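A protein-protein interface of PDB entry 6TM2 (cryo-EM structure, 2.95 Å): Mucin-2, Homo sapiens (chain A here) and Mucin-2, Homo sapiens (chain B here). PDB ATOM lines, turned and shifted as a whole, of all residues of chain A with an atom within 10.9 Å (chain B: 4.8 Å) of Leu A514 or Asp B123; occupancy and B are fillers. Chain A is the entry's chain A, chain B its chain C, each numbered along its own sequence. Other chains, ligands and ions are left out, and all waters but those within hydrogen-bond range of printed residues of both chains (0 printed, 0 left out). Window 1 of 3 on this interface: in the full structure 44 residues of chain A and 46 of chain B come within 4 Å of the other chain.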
ATOM      1  N   THR A 381       3.735 -17.302  -7.407  1.00  0.00           N
ATOM      2  CA  THR A 381       4.572 -16.175  -7.779  1.00  0.00           C
ATOM      3  C   THR A 381       4.714 -15.224  -6.595  1.00  0.00           C
ATOM      4  O   THR A 381       4.189 -15.461  -5.508  1.00  0.00           O
ATOM      5  CB  THR A 381       3.992 -15.451  -8.990  1.00  0.00           C
ATOM      6  OG1 THR A 381       2.740 -14.869  -8.640  1.00  0.00           O
ATOM      7  CG2 THR A 381       3.763 -16.410 -10.126  1.00  0.00           C
ATOM      8  N   PHE A 382       5.418 -14.113  -6.809  1.00  0.00           N
ATOM      9  CA  PHE A 382       5.569 -13.132  -5.744  1.00  0.00           C
ATOM     10  C   PHE A 382       4.279 -12.380  -5.436  1.00  0.00           C
ATOM     11  O   PHE A 382       4.199 -11.736  -4.389  1.00  0.00           O
ATOM     12  CB  PHE A 382       6.631 -12.098  -6.084  1.00  0.00           C
ATOM     13  CG  PHE A 382       8.035 -12.608  -6.095  1.00  0.00           C
ATOM     14  CD1 PHE A 382       8.707 -12.845  -4.918  1.00  0.00           C
ATOM     15  CD2 PHE A 382       8.725 -12.733  -7.279  1.00  0.00           C
ATOM     16  CE1 PHE A 382      10.013 -13.279  -4.924  1.00  0.00           C
ATOM     17  CE2 PHE A 382      10.038 -13.155  -7.287  1.00  0.00           C
ATOM     18  CZ  PHE A 382      10.676 -13.436  -6.105  1.00  0.00           C
ATOM     19  N   ASP A 383       3.286 -12.431  -6.317  1.00  0.00           N
ATOM     20  CA  ASP A 383       2.066 -11.641  -6.205  1.00  0.00           C
ATOM     21  C   ASP A 383       0.834 -12.522  -6.091  1.00  0.00           C
ATOM     22  O   ASP A 383      -0.214 -12.209  -6.644  1.00  0.00           O
ATOM     23  CB  ASP A 383       1.913 -10.705  -7.399  1.00  0.00           C
ATOM     24  CG  ASP A 383       2.931  -9.609  -7.403  1.00  0.00           C
ATOM     25  OD1 ASP A 383       3.380  -9.228  -6.311  1.00  0.00           O
ATOM     26  OD2 ASP A 383       3.278  -9.117  -8.488  1.00  0.00           O
ATOM     27  N   GLY A 384       0.933 -13.617  -5.361  1.00  0.00           N
ATOM     28  CA  GLY A 384      -0.129 -14.611  -5.348  1.00  0.00           C
ATOM     29  C   GLY A 384       0.063 -15.550  -6.510  1.00  0.00           C
ATOM     30  O   GLY A 384       1.175 -15.992  -6.760  1.00  0.00           O
ATOM     31  N   LYS A 385      -1.026 -15.840  -7.228  1.00  0.00           N
ATOM     32  CA  LYS A 385      -1.003 -16.435  -8.569  1.00  0.00           C
ATOM     33  C   LYS A 385      -0.330 -17.816  -8.565  1.00  0.00           C
ATOM     34  O   LYS A 385       0.827 -17.985  -8.937  1.00  0.00           O
ATOM     35  CB  LYS A 385      -0.349 -15.458  -9.555  1.00  0.00           C
ATOM     36  CG  LYS A 385      -0.382 -15.845 -11.023  1.00  0.00           C
ATOM     37  CD  LYS A 385      -1.768 -15.717 -11.570  1.00  0.00           C
ATOM     38  CE  LYS A 385      -1.782 -15.938 -13.056  1.00  0.00           C
ATOM     39  NZ  LYS A 385      -3.161 -15.819 -13.575  1.00  0.00           N
ATOM     40  N   THR A 386      -1.048 -18.783  -8.010  1.00  0.00           N
ATOM     41  CA  THR A 386      -0.581 -20.161  -7.969  1.00  0.00           C
ATOM     42  C   THR A 386      -0.961 -20.884  -9.260  1.00  0.00           C
ATOM     43  O   THR A 386      -2.085 -20.745  -9.743  1.00  0.00           O
ATOM     44  CB  THR A 386      -1.184 -20.876  -6.754  1.00  0.00           C
ATOM     45  OG1 THR A 386      -0.873 -20.138  -5.568  1.00  0.00           O
ATOM     46  CG2 THR A 386      -0.604 -22.271  -6.588  1.00  0.00           C
ATOM     47  N   GLN A 498      11.480  -5.494  -0.835  1.00  0.00           N
ATOM     48  CA  GLN A 498      10.531  -4.693  -1.590  1.00  0.00           C
ATOM     49  C   GLN A 498      11.232  -3.568  -2.351  1.00  0.00           C
ATOM     50  O   GLN A 498      10.598  -2.859  -3.135  1.00  0.00           O
ATOM     51  CB  GLN A 498       9.440  -4.185  -0.626  1.00  0.00           C
ATOM     52  CG  GLN A 498       8.193  -3.573  -1.252  1.00  0.00           C
ATOM     53  CD  GLN A 498       7.119  -3.249  -0.246  1.00  0.00           C
ATOM     54  OE1 GLN A 498       7.286  -3.474   0.947  1.00  0.00           O
ATOM     55  NE2 GLN A 498       6.003  -2.714  -0.723  1.00  0.00           N
ATOM     56  N   GLN A 501      11.216  -4.289  -6.490  1.00  0.00           N
ATOM     57  CA  GLN A 501       9.805  -4.448  -6.808  1.00  0.00           C
ATOM     58  C   GLN A 501       9.571  -3.949  -8.226  1.00  0.00           C
ATOM     59  O   GLN A 501       9.758  -2.762  -8.511  1.00  0.00           O
ATOM     60  CB  GLN A 501       8.932  -3.692  -5.807  1.00  0.00           C
ATOM     61  CG  GLN A 501       7.465  -4.023  -5.900  1.00  0.00           C
ATOM     62  CD  GLN A 501       6.626  -3.325  -4.871  1.00  0.00           C
ATOM     63  OE1 GLN A 501       7.114  -2.477  -4.128  1.00  0.00           O
ATOM     64  NE2 GLN A 501       5.357  -3.703  -4.791  1.00  0.00           N
ATOM     65  N   GLY A 502       9.159  -4.854  -9.108  1.00  0.00           N
ATOM     66  CA  GLY A 502       9.097  -4.544 -10.519  1.00  0.00           C
ATOM     67  C   GLY A 502      10.416  -4.668 -11.244  1.00  0.00           C
ATOM     68  O   GLY A 502      10.576  -4.076 -12.314  1.00  0.00           O
ATOM     69  N   VAL A 504      12.322  -7.917 -11.454  1.00  0.00           N
ATOM     70  CA  VAL A 504      12.690  -9.317 -11.638  1.00  0.00           C
ATOM     71  C   VAL A 504      11.832  -9.937 -12.728  1.00  0.00           C
ATOM     72  O   VAL A 504      10.718  -9.493 -13.005  1.00  0.00           O
ATOM     73  CB  VAL A 504      12.568 -10.157 -10.351  1.00  0.00           C
ATOM     74  CG1 VAL A 504      13.635  -9.787  -9.362  1.00  0.00           C
ATOM     75  CG2 VAL A 504      11.207  -9.942  -9.730  1.00  0.00           C
ATOM     76  N   CYS A 508       8.652 -16.654 -11.582  1.00  0.00           N
ATOM     77  CA  CYS A 508       8.085 -16.095 -10.371  1.00  0.00           C
ATOM     78  C   CYS A 508       7.386 -14.766 -10.598  1.00  0.00           C
ATOM     79  O   CYS A 508       6.966 -14.136  -9.629  1.00  0.00           O
ATOM     80  CB  CYS A 508       9.171 -15.930  -9.314  1.00  0.00           C
ATOM     81  SG  CYS A 508       9.820 -17.455  -8.617  1.00  0.00           S
ATOM     82  N   GLY A 509       7.251 -14.327 -11.838  1.00  0.00           N
ATOM     83  CA  GLY A 509       6.562 -13.092 -12.126  1.00  0.00           C
ATOM     84  C   GLY A 509       7.470 -11.893 -12.011  1.00  0.00           C
ATOM     85  O   GLY A 509       8.693 -11.999 -11.929  1.00  0.00           O
ATOM     86  N   ASN A 510       6.852 -10.715 -12.003  1.00  0.00           N
ATOM     87  CA  ASN A 510       7.614  -9.479 -11.952  1.00  0.00           C
ATOM     88  C   ASN A 510       7.472  -8.684 -10.664  1.00  0.00           C
ATOM     89  O   ASN A 510       8.222  -7.718 -10.497  1.00  0.00           O
ATOM     90  CB  ASN A 510       7.283  -8.579 -13.154  1.00  0.00           C
ATOM     91  CG  ASN A 510       5.821  -8.247 -13.269  1.00  0.00           C
ATOM     92  OD1 ASN A 510       5.010  -8.625 -12.437  1.00  0.00           O
ATOM     93  ND2 ASN A 510       5.478  -7.516 -14.315  1.00  0.00           N
ATOM     94  N   PHE A 511       6.552  -9.064  -9.763  1.00  0.00           N
ATOM     95  CA  PHE A 511       6.439  -8.511  -8.406  1.00  0.00           C
ATOM     96  C   PHE A 511       6.184  -7.001  -8.449  1.00  0.00           C
ATOM     97  O   PHE A 511       7.062  -6.183  -8.206  1.00  0.00           O
ATOM     98  CB  PHE A 511       7.673  -8.932  -7.587  1.00  0.00           C
ATOM     99  CG  PHE A 511       7.729  -8.416  -6.171  1.00  0.00           C
ATOM    100  CD1 PHE A 511       6.734  -8.708  -5.257  1.00  0.00           C
ATOM    101  CD2 PHE A 511       8.892  -7.836  -5.701  1.00  0.00           C
ATOM    102  CE1 PHE A 511       6.827  -8.288  -3.946  1.00  0.00           C
ATOM    103  CE2 PHE A 511       8.999  -7.432  -4.387  1.00  0.00           C
ATOM    104  CZ  PHE A 511       7.964  -7.658  -3.513  1.00  0.00           C
ATOM    105  N   ASN A 512       4.972  -6.662  -8.903  1.00  0.00           N
ATOM    106  CA  ASN A 512       4.541  -5.274  -9.018  1.00  0.00           C
ATOM    107  C   ASN A 512       3.193  -4.976  -8.365  1.00  0.00           C
ATOM    108  O   ASN A 512       2.702  -3.852  -8.487  1.00  0.00           O
ATOM    109  CB  ASN A 512       4.507  -4.839 -10.493  1.00  0.00           C
ATOM    110  CG  ASN A 512       3.580  -5.689 -11.355  1.00  0.00           C
ATOM    111  OD1 ASN A 512       2.919  -6.610 -10.887  1.00  0.00           O
ATOM    112  ND2 ASN A 512       3.511  -5.347 -12.629  1.00  0.00           N
ATOM    113  N   GLY A 513       2.571  -5.942  -7.693  1.00  0.00           N
ATOM    114  CA  GLY A 513       1.309  -5.745  -7.027  1.00  0.00           C
ATOM    115  C   GLY A 513       0.117  -6.353  -7.738  1.00  0.00           C
ATOM    116  O   GLY A 513      -0.788  -6.866  -7.077  1.00  0.00           O
ATOM    117  N   LEU A 514       0.090  -6.298  -9.060  1.00  0.00           N
ATOM    118  CA  LEU A 514      -0.936  -6.934  -9.873  1.00  0.00           C
ATOM    119  C   LEU A 514      -0.530  -8.367 -10.189  1.00  0.00           C
ATOM    120  O   LEU A 514       0.646  -8.647 -10.411  1.00  0.00           O
ATOM    121  CB  LEU A 514      -1.128  -6.146 -11.169  1.00  0.00           C
ATOM    122  CG  LEU A 514      -2.139  -6.538 -12.240  1.00  0.00           C
ATOM    123  CD1 LEU A 514      -3.558  -6.415 -11.774  1.00  0.00           C
ATOM    124  CD2 LEU A 514      -1.895  -5.681 -13.453  1.00  0.00           C
ATOM    125  N   GLU A 515      -1.496  -9.279 -10.205  1.00  0.00           N
ATOM    126  CA  GLU A 515      -1.218 -10.654 -10.595  1.00  0.00           C
ATOM    127  C   GLU A 515      -1.843 -11.008 -11.933  1.00  0.00           C
ATOM    128  O   GLU A 515      -1.790 -12.168 -12.343  1.00  0.00           O
ATOM    129  CB  GLU A 515      -1.694 -11.641  -9.531  1.00  0.00           C
ATOM    130  CG  GLU A 515      -3.189 -11.733  -9.384  1.00  0.00           C
ATOM    131  CD  GLU A 515      -3.610 -12.695  -8.301  1.00  0.00           C
ATOM    132  OE1 GLU A 515      -2.727 -13.260  -7.640  1.00  0.00           O
ATOM    133  OE2 GLU A 515      -4.826 -12.899  -8.116  1.00  0.00           O
ATOM    134  N   GLY A 516      -2.442 -10.037 -12.622  1.00  0.00           N
ATOM    135  CA  GLY A 516      -2.943 -10.292 -13.955  1.00  0.00           C
ATOM    136  C   GLY A 516      -1.858 -10.317 -15.005  1.00  0.00           C
ATOM    137  O   GLY A 516      -2.033 -10.934 -16.057  1.00  0.00           O
ATOM    138  N   ASP A 517      -0.731  -9.656 -14.744  1.00  0.00           N
ATOM    139  CA  ASP A 517       0.370  -9.603 -15.691  1.00  0.00           C
ATOM    140  C   ASP A 517       1.552 -10.470 -15.285  1.00  0.00           C
ATOM    141  O   ASP A 517       2.682 -10.180 -15.678  1.00  0.00           O
ATOM    142  CB  ASP A 517       0.839  -8.164 -15.905  1.00  0.00           C
ATOM    143  CG  ASP A 517       1.332  -7.494 -14.632  1.00  0.00           C
ATOM    144  OD1 ASP A 517       1.216  -8.064 -13.530  1.00  0.00           O
ATOM    145  OD2 ASP A 517       1.868  -6.375 -14.747  1.00  0.00           O
ATOM    146  N   ASP A 518       1.333 -11.506 -14.481  1.00  0.00           N
ATOM    147  CA  ASP A 518       2.451 -12.391 -14.191  1.00  0.00           C
ATOM    148  C   ASP A 518       2.747 -13.321 -15.351  1.00  0.00           C
ATOM    149  O   ASP A 518       3.899 -13.725 -15.524  1.00  0.00           O
ATOM    150  CB  ASP A 518       2.215 -13.193 -12.914  1.00  0.00           C
ATOM    151  CG  ASP A 518       2.446 -12.385 -11.660  1.00  0.00           C
ATOM    152  OD1 ASP A 518       3.254 -11.448 -11.684  1.00  0.00           O
ATOM    153  OD2 ASP A 518       1.851 -12.726 -10.631  1.00  0.00           O
ATOM    154  N   PHE A 519       1.749 -13.638 -16.177  1.00  0.00           N
ATOM    155  CA  PHE A 519       1.969 -14.445 -17.368  1.00  0.00           C
ATOM    156  C   PHE A 519       2.383 -13.615 -18.572  1.00  0.00           C
ATOM    157  O   PHE A 519       2.206 -14.060 -19.704  1.00  0.00           O
ATOM    158  CB  PHE A 519       0.729 -15.265 -17.714  1.00  0.00           C
ATOM    159  CG  PHE A 519       0.457 -16.396 -16.769  1.00  0.00           C
ATOM    160  CD1 PHE A 519       1.413 -16.819 -15.862  1.00  0.00           C
ATOM    161  CD2 PHE A 519      -0.743 -17.062 -16.817  1.00  0.00           C
ATOM    162  CE1 PHE A 519       1.155 -17.847 -15.010  1.00  0.00           C
ATOM    163  CE2 PHE A 519      -1.000 -18.094 -15.963  1.00  0.00           C
ATOM    164  CZ  PHE A 519      -0.045 -18.489 -15.065  1.00  0.00           C
ATOM    165  N   LYS A 520       2.922 -12.426 -18.349  1.00  0.00           N
ATOM    166  CA  LYS A 520       3.443 -11.577 -19.408  1.00  0.00           C
ATOM    167  C   LYS A 520       4.838 -12.040 -19.792  1.00  0.00           C
ATOM    168  O   LYS A 520       5.752 -12.016 -18.965  1.00  0.00           O
ATOM    169  CB  LYS A 520       3.479 -10.137 -18.924  1.00  0.00           C
ATOM    170  CG  LYS A 520       3.954  -9.143 -19.925  1.00  0.00           C
ATOM    171  CD  LYS A 520       3.919  -7.774 -19.305  1.00  0.00           C
ATOM    172  CE  LYS A 520       4.443  -6.725 -20.245  1.00  0.00           C
ATOM    173  NZ  LYS A 520       4.429  -5.384 -19.602  1.00  0.00           N
ATOM    174  N   VAL A 526       0.694 -10.836 -22.614  1.00  0.00           N
ATOM    175  CA  VAL A 526       0.306 -11.778 -21.572  1.00  0.00           C
ATOM    176  C   VAL A 526      -0.255 -13.045 -22.203  1.00  0.00           C
ATOM    177  O   VAL A 526      -1.121 -12.986 -23.083  1.00  0.00           O
ATOM    178  CB  VAL A 526      -0.720 -11.118 -20.637  1.00  0.00           C
ATOM    179  CG1 VAL A 526      -1.242 -12.085 -19.621  1.00  0.00           C
ATOM    180  CG2 VAL A 526      -0.105  -9.933 -19.941  1.00  0.00           C
ATOM    181  N   THR B 121     -13.068  -8.808 -10.134  1.00  0.00           N
ATOM    182  CA  THR B 121     -13.026  -7.365  -9.967  1.00  0.00           C
ATOM    183  C   THR B 121     -12.473  -6.702 -11.229  1.00  0.00           C
ATOM    184  O   THR B 121     -12.051  -7.371 -12.171  1.00  0.00           O
ATOM    185  CB  THR B 121     -12.199  -6.989  -8.742  1.00  0.00           C
ATOM    186  OG1 THR B 121     -10.839  -7.366  -8.939  1.00  0.00           O
ATOM    187  CG2 THR B 121     -12.718  -7.703  -7.526  1.00  0.00           C
ATOM    188  N   PHE B 122     -12.506  -5.362 -11.254  1.00  0.00           N
ATOM    189  CA  PHE B 122     -11.971  -4.595 -12.382  1.00  0.00           C
ATOM    190  C   PHE B 122     -10.488  -4.842 -12.624  1.00  0.00           C
ATOM    191  O   PHE B 122     -10.012  -4.621 -13.738  1.00  0.00           O
ATOM    192  CB  PHE B 122     -12.148  -3.085 -12.181  1.00  0.00           C
ATOM    193  CG  PHE B 122     -13.552  -2.576 -12.340  1.00  0.00           C
ATOM    194  CD1 PHE B 122     -14.079  -2.375 -13.588  1.00  0.00           C
ATOM    195  CD2 PHE B 122     -14.305  -2.210 -11.246  1.00  0.00           C
ATOM    196  CE1 PHE B 122     -15.353  -1.887 -13.747  1.00  0.00           C
ATOM    197  CE2 PHE B 122     -15.576  -1.724 -11.405  1.00  0.00           C
ATOM    198  CZ  PHE B 122     -16.098  -1.567 -12.662  1.00  0.00           C
ATOM    199  N   ASP B 123      -9.748  -5.259 -11.600  1.00  0.00           N
ATOM    200  CA  ASP B 123      -8.333  -5.572 -11.690  1.00  0.00           C
ATOM    201  C   ASP B 123      -8.070  -7.063 -11.787  1.00  0.00           C
ATOM    202  O   ASP B 123      -6.913  -7.478 -11.764  1.00  0.00           O
ATOM    203  CB  ASP B 123      -7.598  -4.988 -10.492  1.00  0.00           C
ATOM    204  CG  ASP B 123      -7.565  -3.484 -10.518  1.00  0.00           C
ATOM    205  OD1 ASP B 123      -7.576  -2.910 -11.617  1.00  0.00           O
ATOM    206  OD2 ASP B 123      -7.536  -2.870  -9.439  1.00  0.00           O
ATOM    207  N   GLY B 124      -9.114  -7.874 -11.883  1.00  0.00           N
ATOM    208  CA  GLY B 124      -8.968  -9.278 -12.198  1.00  0.00           C
ATOM    209  C   GLY B 124      -8.690 -10.181 -11.023  1.00  0.00           C
ATOM    210  O   GLY B 124      -7.786 -11.010 -11.091  1.00  0.00           O
ATOM    211  N   LYS B 125      -9.471 -10.065  -9.958  1.00  0.00           N
ATOM    212  CA  LYS B 125      -9.305 -10.886  -8.768  1.00  0.00           C
ATOM    213  C   LYS B 125     -10.563 -11.713  -8.570  1.00  0.00           C
ATOM    214  O   LYS B 125     -11.655 -11.156  -8.465  1.00  0.00           O
ATOM    215  CB  LYS B 125      -9.029 -10.008  -7.555  1.00  0.00           C
ATOM    216  CG  LYS B 125      -8.712 -10.756  -6.305  1.00  0.00           C
ATOM    217  CD  LYS B 125      -8.266  -9.814  -5.240  1.00  0.00           C
ATOM    218  CE  LYS B 125      -7.812 -10.573  -4.024  1.00  0.00           C
ATOM    219  NZ  LYS B 125      -7.282  -9.627  -3.012  1.00  0.00           N
ATOM    220  N   ASN B 245     -11.417  -1.130  -7.027  1.00  0.00           N
ATOM    221  CA  ASN B 245     -11.227   0.296  -7.241  1.00  0.00           C
ATOM    222  C   ASN B 245     -10.583   0.703  -8.559  1.00  0.00           C
ATOM    223  O   ASN B 245     -10.381   1.901  -8.759  1.00  0.00           O
ATOM    224  CB  ASN B 245     -10.432   0.910  -6.078  1.00  0.00           C
ATOM    225  CG  ASN B 245      -9.112   0.229  -5.826  1.00  0.00           C
ATOM    226  OD1 ASN B 245      -8.702  -0.667  -6.547  1.00  0.00           O
ATOM    227  ND2 ASN B 245      -8.438   0.653  -4.777  1.00  0.00           N
ATOM    228  N   PHE B 246     -10.250  -0.244  -9.441  1.00  0.00           N
ATOM    229  CA  PHE B 246      -9.919  -0.003 -10.854  1.00  0.00           C
ATOM    230  C   PHE B 246      -8.686   0.896 -11.003  1.00  0.00           C
ATOM    231  O   PHE B 246      -8.702   1.940 -11.643  1.00  0.00           O
ATOM    232  CB  PHE B 246     -11.174   0.513 -11.586  1.00  0.00           C
ATOM    233  CG  PHE B 246     -11.024   0.720 -13.076  1.00  0.00           C
ATOM    234  CD1 PHE B 246     -10.696  -0.317 -13.921  1.00  0.00           C
ATOM    235  CD2 PHE B 246     -11.415   1.909 -13.644  1.00  0.00           C
ATOM    236  CE1 PHE B 246     -10.606  -0.114 -15.278  1.00  0.00           C
ATOM    237  CE2 PHE B 246     -11.349   2.104 -15.005  1.00  0.00           C
ATOM    238  CZ  PHE B 246     -10.943   1.099 -15.816  1.00  0.00           C
ATOM    239  N   ASP B 247      -7.589   0.464 -10.373  1.00  0.00           N
ATOM    240  CA  ASP B 247      -6.326   1.183 -10.476  1.00  0.00           C
ATOM    241  C   ASP B 247      -5.171   0.302 -10.934  1.00  0.00           C
ATOM    242  O   ASP B 247      -4.021   0.636 -10.640  1.00  0.00           O
ATOM    243  CB  ASP B 247      -5.966   1.883  -9.162  1.00  0.00           C
ATOM    244  CG  ASP B 247      -5.853   0.943  -7.990  1.00  0.00           C
ATOM    245  OD1 ASP B 247      -6.172  -0.249  -8.113  1.00  0.00           O
ATOM    246  OD2 ASP B 247      -5.423   1.404  -6.921  1.00  0.00           O
ATOM    247  N   HIS B 248      -5.475  -0.811 -11.620  1.00  0.00           N
ATOM    248  CA  HIS B 248      -4.487  -1.685 -12.260  1.00  0.00           C
ATOM    249  C   HIS B 248      -3.456  -2.213 -11.269  1.00  0.00           C
ATOM    250  O   HIS B 248      -2.259  -2.236 -11.546  1.00  0.00           O
ATOM    251  CB  HIS B 248      -3.815  -0.976 -13.433  1.00  0.00           C
ATOM    252  CG  HIS B 248      -4.787  -0.395 -14.410  1.00  0.00           C
ATOM    253  ND1 HIS B 248      -5.419  -1.158 -15.367  1.00  0.00           N
ATOM    254  CD2 HIS B 248      -5.257   0.864 -14.565  1.00  0.00           C
ATOM    255  CE1 HIS B 248      -6.228  -0.393 -16.075  1.00  0.00           C
ATOM    256  NE2 HIS B 248      -6.149   0.839 -15.608  1.00  0.00           N
ATOM    257  N   ARG B 249      -3.935  -2.639 -10.109  1.00  0.00           N
ATOM    258  CA  ARG B 249      -3.092  -3.100  -9.014  1.00  0.00           C
ATOM    259  C   ARG B 249      -4.026  -3.874  -8.094  1.00  0.00           C
ATOM    260  O   ARG B 249      -4.888  -3.268  -7.462  1.00  0.00           O
ATOM    261  CB  ARG B 249      -2.437  -1.896  -8.334  1.00  0.00           C
ATOM    262  CG  ARG B 249      -1.516  -2.108  -7.161  1.00  0.00           C
ATOM    263  CD  ARG B 249      -2.300  -1.842  -5.915  1.00  0.00           C
ATOM    264  NE  ARG B 249      -1.549  -1.890  -4.668  1.00  0.00           N
ATOM    265  CZ  ARG B 249      -0.993  -0.828  -4.101  1.00  0.00           C
ATOM    266  NH1 ARG B 249      -1.111   0.362  -4.671  1.00  0.00           N
ATOM    267  NH2 ARG B 249      -0.343  -0.948  -2.956  1.00  0.00           N
ATOM    268  N   SER B 250      -3.888  -5.194  -8.030  1.00  0.00           N
ATOM    269  CA  SER B 250      -4.961  -6.009  -7.479  1.00  0.00           C
ATOM    270  C   SER B 250      -4.743  -6.443  -6.044  1.00  0.00           C
ATOM    271  O   SER B 250      -5.560  -7.202  -5.526  1.00  0.00           O
ATOM    272  CB  SER B 250      -5.180  -7.260  -8.316  1.00  0.00           C
ATOM    273  OG  SER B 250      -4.116  -8.165  -8.135  1.00  0.00           O
ATOM    274  N   ASP B 253      -7.734  -4.677  -3.703  1.00  0.00           N
ATOM    275  CA  ASP B 253      -9.154  -4.758  -4.014  1.00  0.00           C
ATOM    276  C   ASP B 253     -10.003  -5.149  -2.818  1.00  0.00           C
ATOM    277  O   ASP B 253     -11.210  -4.907  -2.834  1.00  0.00           O
ATOM    278  CB  ASP B 253      -9.424  -5.742  -5.145  1.00  0.00           C
ATOM    279  CG  ASP B 253      -9.017  -5.211  -6.485  1.00  0.00           C
ATOM    280  OD1 ASP B 253      -8.983  -3.983  -6.653  1.00  0.00           O
ATOM    281  OD2 ASP B 253      -8.804  -6.025  -7.396  1.00  0.00           O
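The backbone NH (N) of His B248 sits at hydrogen-bond distance from the side-chain carboxylate (OD1) of Asp B123. N of Lys A385 sits at hydrogen-bond distance from OE1 of Glu A515. OD2 of Asp A383 is in hydrogen-bond range of N of Gly A513 (3.3 Å).
Of the 24 printed residues of chain A, 3 touch a printed residue of chain B. Hydrophobic or aromatic side chains of chain A that line the printed part of chain B: Leu A514. Among the printed residues, 5 pairs touch across the chains.
Of the printed residues of chain B, Leu A514 touches Asp B123 (3.5 Å), His B248 (3.95 Å) and Ser B250 (3.8 Å). Of chain A, only Leu A514 comes within 4 Å of Asp B123. No residue of chain A comes within 4 Å of Gly B124. No residue of chain A comes within 4 Å of Asn B245. Of chain A, only Gly A513, Leu A514 and Glu A515 come within 4 Å of Ser B250. Of the printed residues of chain A, His B248 touches Leu A514. Of the printed residues of chain B, Gly A513 touches Ser B250. The nearest printed residue of chain A that does not touch His B248 is Asn A512 (6.0 Å).
Among the printed residues, merely in contact across the chains: Leu A514 with Asp B123 (3.5 Å), Glu A515 with Ser B250 (3.5 Å), Gly A513 with Ser B250 (3.6 Å), Leu A514 with Ser B250 (3.8 Å) and Leu A514 with His B248 (3.95 Å).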
